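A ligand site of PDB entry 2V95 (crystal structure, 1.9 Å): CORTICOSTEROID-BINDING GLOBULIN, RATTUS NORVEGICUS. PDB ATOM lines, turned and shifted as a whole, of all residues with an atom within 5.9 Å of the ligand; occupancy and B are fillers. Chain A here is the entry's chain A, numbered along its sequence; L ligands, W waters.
Water W3 lies within hydrogen-bond range of O3 of the ligand (2.6 Å), NE1 of Trp 359 (2.9 Å) and O of Lys 356 (3.3 Å). Water W2 lies within hydrogen-bond range of the side-chain amide oxygen of Gln 221, an oxygen (O5) of the ligand and the backbone carbonyl oxygen of Gly 256. Water W1 lies within hydrogen-bond range of O of Asp 253, O2 of the ligand and N of Lys 257.
O4 of the ligand lies within hydrogen-bond range of NE2 of Gln 221, at 2.9 Å. The side-chain carboxylate (OD1) of Asp 253 lies within hydrogen-bond range of an oxygen (O2) of the ligand, at 2.6 Å.
The backbone carbonyl oxygen (O) of Lys 356 lies within hydrogen-bond range of the guanidinium group (NH2) of Arg 7, at 3.0 Å. O of Thr 229 sits at hydrogen-bond distance from N of Phe 354, 3.0 Å away. NE2 of Gln 221 sits at hydrogen-bond distance from OG1 of Thr 229 (3.0 Å). The side-chain carboxylate of Asp 253 lies within salt-bridge range of the side-chain amino group of Lys 257 (3.2 Å). The indole nitrogen (NE1) of Trp 359 lies close to the backbone carbonyl oxygen (O) of Lys 356.
Ala 10 touches the ligand. Pro 11 touches the ligand (CG to O1, 3.5 Å). CG1 of Val 14 touches C6 of the ligand, 3.97 Å away. CG2 of Thr 229 touches C16 of the ligand, 3.9 Å away. CZ of Phe 231 touches O4 of the ligand (3.7 Å). Arg 249 touches the ligand (CD to C3, 3.6 Å). O of Ile 252 touches C18 of the ligand, 3.97 Å away. Phe 354 touches the ligand. CA of Lys 356 touches O3 of the ligand, 3.5 Å away. Trp 359 touches the ligand. Hydrophobic or aromatic side chains that line the ligand: Ala 10, Pro 11, Val 14, Phe 231, Ile 252, Phe 354 and Trp 359.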
ATOM      1  N   ARG A   7      -9.845  14.245  20.123  1.00  0.00           N
ATOM      2  CA  ARG A   7      -9.640  13.875  18.722  1.00  0.00           C
ATOM      3  C   ARG A   7     -10.532  14.648  17.730  1.00  0.00           C
ATOM      4  O   ARG A   7     -10.565  14.339  16.541  1.00  0.00           O
ATOM      5  CB  ARG A   7      -9.844  12.381  18.579  1.00  0.00           C
ATOM      6  CG  ARG A   7      -8.716  11.594  19.203  1.00  0.00           C
ATOM      7  CD  ARG A   7      -9.081  10.165  19.479  1.00  0.00           C
ATOM      8  NE  ARG A   7      -7.913   9.427  19.974  1.00  0.00           N
ATOM      9  CZ  ARG A   7      -7.944   8.157  20.359  1.00  0.00           C
ATOM     10  NH1 ARG A   7      -9.057   7.449  20.292  1.00  0.00           N
ATOM     11  NH2 ARG A   7      -6.841   7.586  20.802  1.00  0.00           N
ATOM     12  N   ALA A  10      -8.965  15.883  14.438  1.00  0.00           N
ATOM     13  CA  ALA A  10      -8.147  14.921  13.681  1.00  0.00           C
ATOM     14  C   ALA A  10      -8.598  14.762  12.219  1.00  0.00           C
ATOM     15  O   ALA A  10      -7.782  14.882  11.315  1.00  0.00           O
ATOM     16  CB  ALA A  10      -8.178  13.530  14.372  1.00  0.00           C
ATOM     17  N   PRO A  11      -9.878  14.463  11.994  1.00  0.00           N
ATOM     18  CA  PRO A  11     -10.293  14.226  10.606  1.00  0.00           C
ATOM     19  C   PRO A  11      -9.937  15.375   9.663  1.00  0.00           C
ATOM     20  O   PRO A  11      -9.349  15.144   8.611  1.00  0.00           O
ATOM     21  CB  PRO A  11     -11.802  14.034  10.715  1.00  0.00           C
ATOM     22  CG  PRO A  11     -12.032  13.598  12.112  1.00  0.00           C
ATOM     23  CD  PRO A  11     -10.994  14.298  12.927  1.00  0.00           C
ATOM     24  N   VAL A  14      -5.898  15.955   9.695  1.00  0.00           N
ATOM     25  CA  VAL A  14      -5.188  14.874   8.992  1.00  0.00           C
ATOM     26  C   VAL A  14      -5.553  14.756   7.479  1.00  0.00           C
ATOM     27  O   VAL A  14      -4.719  14.364   6.672  1.00  0.00           O
ATOM     28  CB  VAL A  14      -5.394  13.526   9.758  1.00  0.00           C
ATOM     29  CG1 VAL A  14      -4.797  12.390   9.018  1.00  0.00           C
ATOM     30  CG2 VAL A  14      -4.738  13.648  11.203  1.00  0.00           C
ATOM     31  N   PHE A  18      -2.338  15.116   4.699  1.00  0.00           N
ATOM     32  CA  PHE A  18      -2.014  14.179   3.625  1.00  0.00           C
ATOM     33  C   PHE A  18      -2.141  14.852   2.237  1.00  0.00           C
ATOM     34  O   PHE A  18      -1.465  14.492   1.289  1.00  0.00           O
ATOM     35  CB  PHE A  18      -2.945  12.938   3.706  1.00  0.00           C
ATOM     36  CG  PHE A  18      -2.482  11.879   4.715  1.00  0.00           C
ATOM     37  CD1 PHE A  18      -1.389  11.090   4.472  1.00  0.00           C
ATOM     38  CD2 PHE A  18      -3.191  11.634   5.869  1.00  0.00           C
ATOM     39  CE1 PHE A  18      -0.985  10.071   5.367  1.00  0.00           C
ATOM     40  CE2 PHE A  18      -2.785  10.628   6.767  1.00  0.00           C
ATOM     41  CZ  PHE A  18      -1.681   9.849   6.507  1.00  0.00           C
ATOM     42  N   GLN A 221       6.232  -0.098  12.336  1.00  0.00           N
ATOM     43  CA  GLN A 221       5.720   0.844  13.352  1.00  0.00           C
ATOM     44  C   GLN A 221       6.661   0.830  14.558  1.00  0.00           C
ATOM     45  O   GLN A 221       6.855  -0.198  15.195  1.00  0.00           O
ATOM     46  CB  GLN A 221       4.282   0.496  13.782  1.00  0.00           C
ATOM     47  CG  GLN A 221       3.703   1.501  14.789  1.00  0.00           C
ATOM     48  CD  GLN A 221       2.197   1.422  14.918  1.00  0.00           C
ATOM     49  OE1 GLN A 221       1.578   0.396  14.591  1.00  0.00           O
ATOM     50  NE2 GLN A 221       1.590   2.504  15.421  1.00  0.00           N
ATOM     51  N   THR A 229       4.256   7.882  17.890  1.00  0.00           N
ATOM     52  CA  THR A 229       4.507   6.661  17.124  1.00  0.00           C
ATOM     53  C   THR A 229       4.995   7.049  15.726  1.00  0.00           C
ATOM     54  O   THR A 229       4.600   8.099  15.177  1.00  0.00           O
ATOM     55  CB  THR A 229       3.254   5.764  17.094  1.00  0.00           C
ATOM     56  OG1 THR A 229       3.584   4.444  16.610  1.00  0.00           O
ATOM     57  CG2 THR A 229       2.134   6.376  16.245  1.00  0.00           C
ATOM     58  N   PHE A 231       5.529   5.644  11.715  1.00  0.00           N
ATOM     59  CA  PHE A 231       5.417   4.691  10.635  1.00  0.00           C
ATOM     60  C   PHE A 231       6.549   4.897   9.630  1.00  0.00           C
ATOM     61  O   PHE A 231       6.663   5.947   9.003  1.00  0.00           O
ATOM     62  CB  PHE A 231       4.061   4.777   9.934  1.00  0.00           C
ATOM     63  CG  PHE A 231       2.909   4.359  10.774  1.00  0.00           C
ATOM     64  CD1 PHE A 231       2.273   5.262  11.610  1.00  0.00           C
ATOM     65  CD2 PHE A 231       2.420   3.063  10.706  1.00  0.00           C
ATOM     66  CE1 PHE A 231       1.191   4.861  12.383  1.00  0.00           C
ATOM     67  CE2 PHE A 231       1.342   2.680  11.462  1.00  0.00           C
ATOM     68  CZ  PHE A 231       0.735   3.577  12.301  1.00  0.00           C
ATOM     69  N   ARG A 249      -6.214   9.292   5.306  1.00  0.00           N
ATOM     70  CA  ARG A 249      -6.696   8.889   6.630  1.00  0.00           C
ATOM     71  C   ARG A 249      -7.322   7.486   6.511  1.00  0.00           C
ATOM     72  O   ARG A 249      -7.195   6.652   7.398  1.00  0.00           O
ATOM     73  CB  ARG A 249      -7.719   9.931   7.155  1.00  0.00           C
ATOM     74  CG  ARG A 249      -8.448   9.552   8.406  1.00  0.00           C
ATOM     75  CD  ARG A 249      -9.156  10.763   9.039  1.00  0.00           C
ATOM     76  NE  ARG A 249     -10.087  11.417   8.123  1.00  0.00           N
ATOM     77  CZ  ARG A 249     -11.418  11.358   8.159  1.00  0.00           C
ATOM     78  NH1 ARG A 249     -12.074  10.721   9.117  1.00  0.00           N
ATOM     79  NH2 ARG A 249     -12.110  12.012   7.237  1.00  0.00           N
ATOM     80  N   ASP A 250      -7.965   7.214   5.401  1.00  0.00           N
ATOM     81  CA  ASP A 250      -8.490   5.858   5.121  1.00  0.00           C
ATOM     82  C   ASP A 250      -7.404   4.762   5.140  1.00  0.00           C
ATOM     83  O   ASP A 250      -7.545   3.728   5.776  1.00  0.00           O
ATOM     84  CB  ASP A 250      -9.112   5.841   3.741  1.00  0.00           C
ATOM     85  CG  ASP A 250     -10.505   6.408   3.726  1.00  0.00           C
ATOM     86  OD1 ASP A 250     -11.243   6.215   4.720  1.00  0.00           O
ATOM     87  OD2 ASP A 250     -10.844   7.063   2.704  1.00  0.00           O
ATOM     88  N   ILE A 252      -3.986   4.947   6.199  1.00  0.00           N
ATOM     89  CA  ILE A 252      -3.284   4.829   7.495  1.00  0.00           C
ATOM     90  C   ILE A 252      -4.085   4.138   8.618  1.00  0.00           C
ATOM     91  O   ILE A 252      -3.481   3.475   9.473  1.00  0.00           O
ATOM     92  CB  ILE A 252      -2.724   6.206   8.010  1.00  0.00           C
ATOM     93  CG1 ILE A 252      -1.741   6.003   9.179  1.00  0.00           C
ATOM     94  CG2 ILE A 252      -3.854   7.100   8.483  1.00  0.00           C
ATOM     95  CD1 ILE A 252      -0.274   5.954   8.743  1.00  0.00           C
ATOM     96  N   ASP A 253      -5.410   4.284   8.609  1.00  0.00           N
ATOM     97  CA  ASP A 253      -6.297   3.571   9.509  1.00  0.00           C
ATOM     98  C   ASP A 253      -6.241   2.061   9.279  1.00  0.00           C
ATOM     99  O   ASP A 253      -6.286   1.272  10.219  1.00  0.00           O
ATOM    100  CB  ASP A 253      -7.747   4.038   9.272  1.00  0.00           C
ATOM    101  CG  ASP A 253      -8.689   3.570  10.341  1.00  0.00           C
ATOM    102  OD1 ASP A 253      -8.500   3.968  11.508  1.00  0.00           O
ATOM    103  OD2 ASP A 253      -9.616   2.803  10.024  1.00  0.00           O
ATOM    104  N   ARG A 254      -6.205   1.683   8.015  1.00  0.00           N
ATOM    105  CA  ARG A 254      -6.041   0.301   7.608  1.00  0.00           C
ATOM    106  C   ARG A 254      -4.711  -0.244   8.070  1.00  0.00           C
ATOM    107  O   ARG A 254      -4.622  -1.276   8.731  1.00  0.00           O
ATOM    108  CB  ARG A 254      -6.095   0.209   6.085  1.00  0.00           C
ATOM    109  CG  ARG A 254      -6.527  -1.138   5.574  1.00  0.00           C
ATOM    110  CD  ARG A 254      -6.705  -1.109   4.053  1.00  0.00           C
ATOM    111  NE  ARG A 254      -6.359  -2.410   3.462  1.00  0.00           N
ATOM    112  CZ  ARG A 254      -5.124  -2.753   3.073  1.00  0.00           C
ATOM    113  NH1 ARG A 254      -4.124  -1.920   3.187  1.00  0.00           N
ATOM    114  NH2 ARG A 254      -4.904  -3.951   2.543  1.00  0.00           N
ATOM    115  N   GLY A 256      -2.599   0.880  10.313  1.00  0.00           N
ATOM    116  CA  GLY A 256      -2.526   0.828  11.772  1.00  0.00           C
ATOM    117  C   GLY A 256      -3.210  -0.395  12.365  1.00  0.00           C
ATOM    118  O   GLY A 256      -2.789  -0.928  13.371  1.00  0.00           O
ATOM    119  N   LYS A 257      -4.292  -0.831  11.725  1.00  0.00           N
ATOM    120  CA  LYS A 257      -5.055  -1.994  12.224  1.00  0.00           C
ATOM    121  C   LYS A 257      -4.474  -3.348  11.823  1.00  0.00           C
ATOM    122  O   LYS A 257      -4.841  -4.368  12.387  1.00  0.00           O
ATOM    123  CB  LYS A 257      -6.527  -1.898  11.784  1.00  0.00           C
ATOM    124  CG  LYS A 257      -7.264  -0.748  12.454  1.00  0.00           C
ATOM    125  CD  LYS A 257      -8.744  -0.710  12.054  1.00  0.00           C
ATOM    126  CE  LYS A 257      -9.365   0.613  12.494  1.00  0.00           C
ATOM    127  NZ  LYS A 257     -10.802   0.754  12.129  1.00  0.00           N
ATOM    128  N   PHE A 354       2.964  10.415  14.287  1.00  0.00           N
ATOM    129  CA  PHE A 354       1.646  10.778  14.791  1.00  0.00           C
ATOM    130  C   PHE A 354       1.598  10.734  16.306  1.00  0.00           C
ATOM    131  O   PHE A 354       2.316   9.971  16.955  1.00  0.00           O
ATOM    132  CB  PHE A 354       0.602   9.789  14.324  1.00  0.00           C
ATOM    133  CG  PHE A 354       0.309   9.806  12.845  1.00  0.00           C
ATOM    134  CD1 PHE A 354       0.903   8.874  12.008  1.00  0.00           C
ATOM    135  CD2 PHE A 354      -0.652  10.671  12.322  1.00  0.00           C
ATOM    136  CE1 PHE A 354       0.600   8.838  10.652  1.00  0.00           C
ATOM    137  CE2 PHE A 354      -0.989  10.647  10.973  1.00  0.00           C
ATOM    138  CZ  PHE A 354      -0.371   9.721  10.120  1.00  0.00           C
ATOM    139  N   ASP A 355       0.660  11.502  16.856  1.00  0.00           N
ATOM    140  CA  ASP A 355       0.274  11.359  18.262  1.00  0.00           C
ATOM    141  C   ASP A 355      -0.922  10.420  18.356  1.00  0.00           C
ATOM    142  O   ASP A 355      -1.991  10.666  17.798  1.00  0.00           O
ATOM    143  CB  ASP A 355      -0.005  12.730  18.886  1.00  0.00           C
ATOM    144  CG  ASP A 355      -0.547  12.649  20.289  1.00  0.00           C
ATOM    145  OD1 ASP A 355      -0.313  11.645  20.987  1.00  0.00           O
ATOM    146  OD2 ASP A 355      -1.230  13.609  20.697  1.00  0.00           O
ATOM    147  N   LYS A 356      -0.735   9.308  19.048  1.00  0.00           N
ATOM    148  CA  LYS A 356      -1.796   8.313  19.205  1.00  0.00           C
ATOM    149  C   LYS A 356      -2.986   8.819  20.020  1.00  0.00           C
ATOM    150  O   LYS A 356      -4.088   8.284  19.882  1.00  0.00           O
ATOM    151  CB  LYS A 356      -1.226   7.050  19.845  1.00  0.00           C
ATOM    152  CG  LYS A 356      -0.266   6.299  18.941  1.00  0.00           C
ATOM    153  CD  LYS A 356      -0.334   4.792  19.155  1.00  0.00           C
ATOM    154  CE  LYS A 356       0.482   4.357  20.339  1.00  0.00           C
ATOM    155  NZ  LYS A 356       0.169   2.907  20.752  1.00  0.00           N
ATOM    156  N   PHE A 357      -2.775   9.837  20.849  1.00  0.00           N
ATOM    157  CA  PHE A 357      -3.820  10.356  21.740  1.00  0.00           C
ATOM    158  C   PHE A 357      -4.758  11.335  21.024  1.00  0.00           C
ATOM    159  O   PHE A 357      -5.975  11.105  20.986  1.00  0.00           O
ATOM    160  CB  PHE A 357      -3.154  10.994  22.970  1.00  0.00           C
ATOM    161  CG  PHE A 357      -4.107  11.544  23.994  1.00  0.00           C
ATOM    162  CD1 PHE A 357      -3.895  12.791  24.556  1.00  0.00           C
ATOM    163  CD2 PHE A 357      -5.214  10.818  24.406  1.00  0.00           C
ATOM    164  CE1 PHE A 357      -4.766  13.307  25.503  1.00  0.00           C
ATOM    165  CE2 PHE A 357      -6.077  11.340  25.356  1.00  0.00           C
ATOM    166  CZ  PHE A 357      -5.854  12.596  25.901  1.00  0.00           C
ATOM    167  N   TRP A 359      -4.487  12.014  17.675  1.00  0.00           N
ATOM    168  CA  TRP A 359      -4.462  11.628  16.244  1.00  0.00           C
ATOM    169  C   TRP A 359      -3.829  12.677  15.324  1.00  0.00           C
ATOM    170  O   TRP A 359      -4.034  12.677  14.113  1.00  0.00           O
ATOM    171  CB  TRP A 359      -5.852  11.193  15.762  1.00  0.00           C
ATOM    172  CG  TRP A 359      -6.283   9.896  16.308  1.00  0.00           C
ATOM    173  CD1 TRP A 359      -5.501   8.946  16.923  1.00  0.00           C
ATOM    174  CD2 TRP A 359      -7.606   9.356  16.260  1.00  0.00           C
ATOM    175  NE1 TRP A 359      -6.274   7.862  17.261  1.00  0.00           N
ATOM    176  CE2 TRP A 359      -7.562   8.086  16.871  1.00  0.00           C
ATOM    177  CE3 TRP A 359      -8.829   9.831  15.771  1.00  0.00           C
ATOM    178  CZ2 TRP A 359      -8.684   7.296  17.003  1.00  0.00           C
ATOM    179  CZ3 TRP A 359      -9.944   9.034  15.893  1.00  0.00           C
ATOM    180  CH2 TRP A 359      -9.869   7.775  16.500  1.00  0.00           C
ATOM    181  N   SER A 360      -2.999  13.527  15.919  1.00  0.00           N
ATOM    182  CA  SER A 360      -2.285  14.571  15.217  1.00  0.00           C
ATOM    183  C   SER A 360      -1.133  14.039  14.381  1.00  0.00           C
ATOM    184  O   SER A 360      -0.471  13.081  14.771  1.00  0.00           O
ATOM    185  CB  SER A 360      -1.717  15.561  16.228  1.00  0.00           C
ATOM    186  OG  SER A 360      -2.720  16.312  16.879  1.00  0.00           O
HETATM  187  C1  LIG L   1      -8.494   7.535  12.926  1.00  0.00           C
HETATM  188  C2  LIG L   1      -9.629   8.474  12.533  1.00  0.00           C
HETATM  189  C3  LIG L   1      -9.152   9.918  12.493  1.00  0.00           C
HETATM  190  C4  LIG L   1      -7.734  10.234  12.310  1.00  0.00           C
HETATM  191  C5  LIG L   1      -6.797   9.273  12.208  1.00  0.00           C
HETATM  192  C6  LIG L   1      -5.398   9.721  11.892  1.00  0.00           C
HETATM  193  C7  LIG L   1      -4.386   9.076  12.811  1.00  0.00           C
HETATM  194  C8  LIG L   1      -4.638   7.586  13.011  1.00  0.00           C
HETATM  195  C9  LIG L   1      -6.083   7.237  13.379  1.00  0.00           C
HETATM  196  C10 LIG L   1      -7.114   7.790  12.357  1.00  0.00           C
HETATM  197  C11 LIG L   1      -5.256   5.264  14.794  1.00  0.00           C
HETATM  198  C12 LIG L   1      -6.292   5.752  13.770  1.00  0.00           C
HETATM  199  C13 LIG L   1      -3.814   5.647  14.442  1.00  0.00           C
HETATM  200  C14 LIG L   1      -3.753   7.142  14.153  1.00  0.00           C
HETATM  201  C15 LIG L   1      -2.283   7.407  14.000  1.00  0.00           C
HETATM  202  C16 LIG L   1      -1.590   6.419  14.944  1.00  0.00           C
HETATM  203  C17 LIG L   1      -2.690   5.553  15.507  1.00  0.00           C
HETATM  204  C18 LIG L   1      -3.419   4.834  13.206  1.00  0.00           C
HETATM  205  C19 LIG L   1      -6.952   7.153  10.974  1.00  0.00           C
HETATM  206  C20 LIG L   1      -2.140   4.174  15.827  1.00  0.00           C
HETATM  207  C21 LIG L   1      -3.017   3.209  16.560  1.00  0.00           C
HETATM  208  O1  LIG L   1      -9.946  10.843  12.621  1.00  0.00           O
HETATM  209  O2  LIG L   1      -6.302   4.850  12.643  1.00  0.00           O
HETATM  210  O3  LIG L   1      -3.072   6.165  16.750  1.00  0.00           O
HETATM  211  O4  LIG L   1      -0.992   3.848  15.530  1.00  0.00           O
HETATM  212  O5  LIG L   1      -2.337   1.959  16.716  1.00  0.00           O
HETATM  213  O   HOH W   1      -5.633   2.102  12.786  1.00  0.00           O
HETATM  214  O   HOH W   2      -0.955   0.414  14.933  1.00  0.00           O
HETATM  215  O   HOH W   3      -4.920   5.499  18.387  1.00  0.00           O
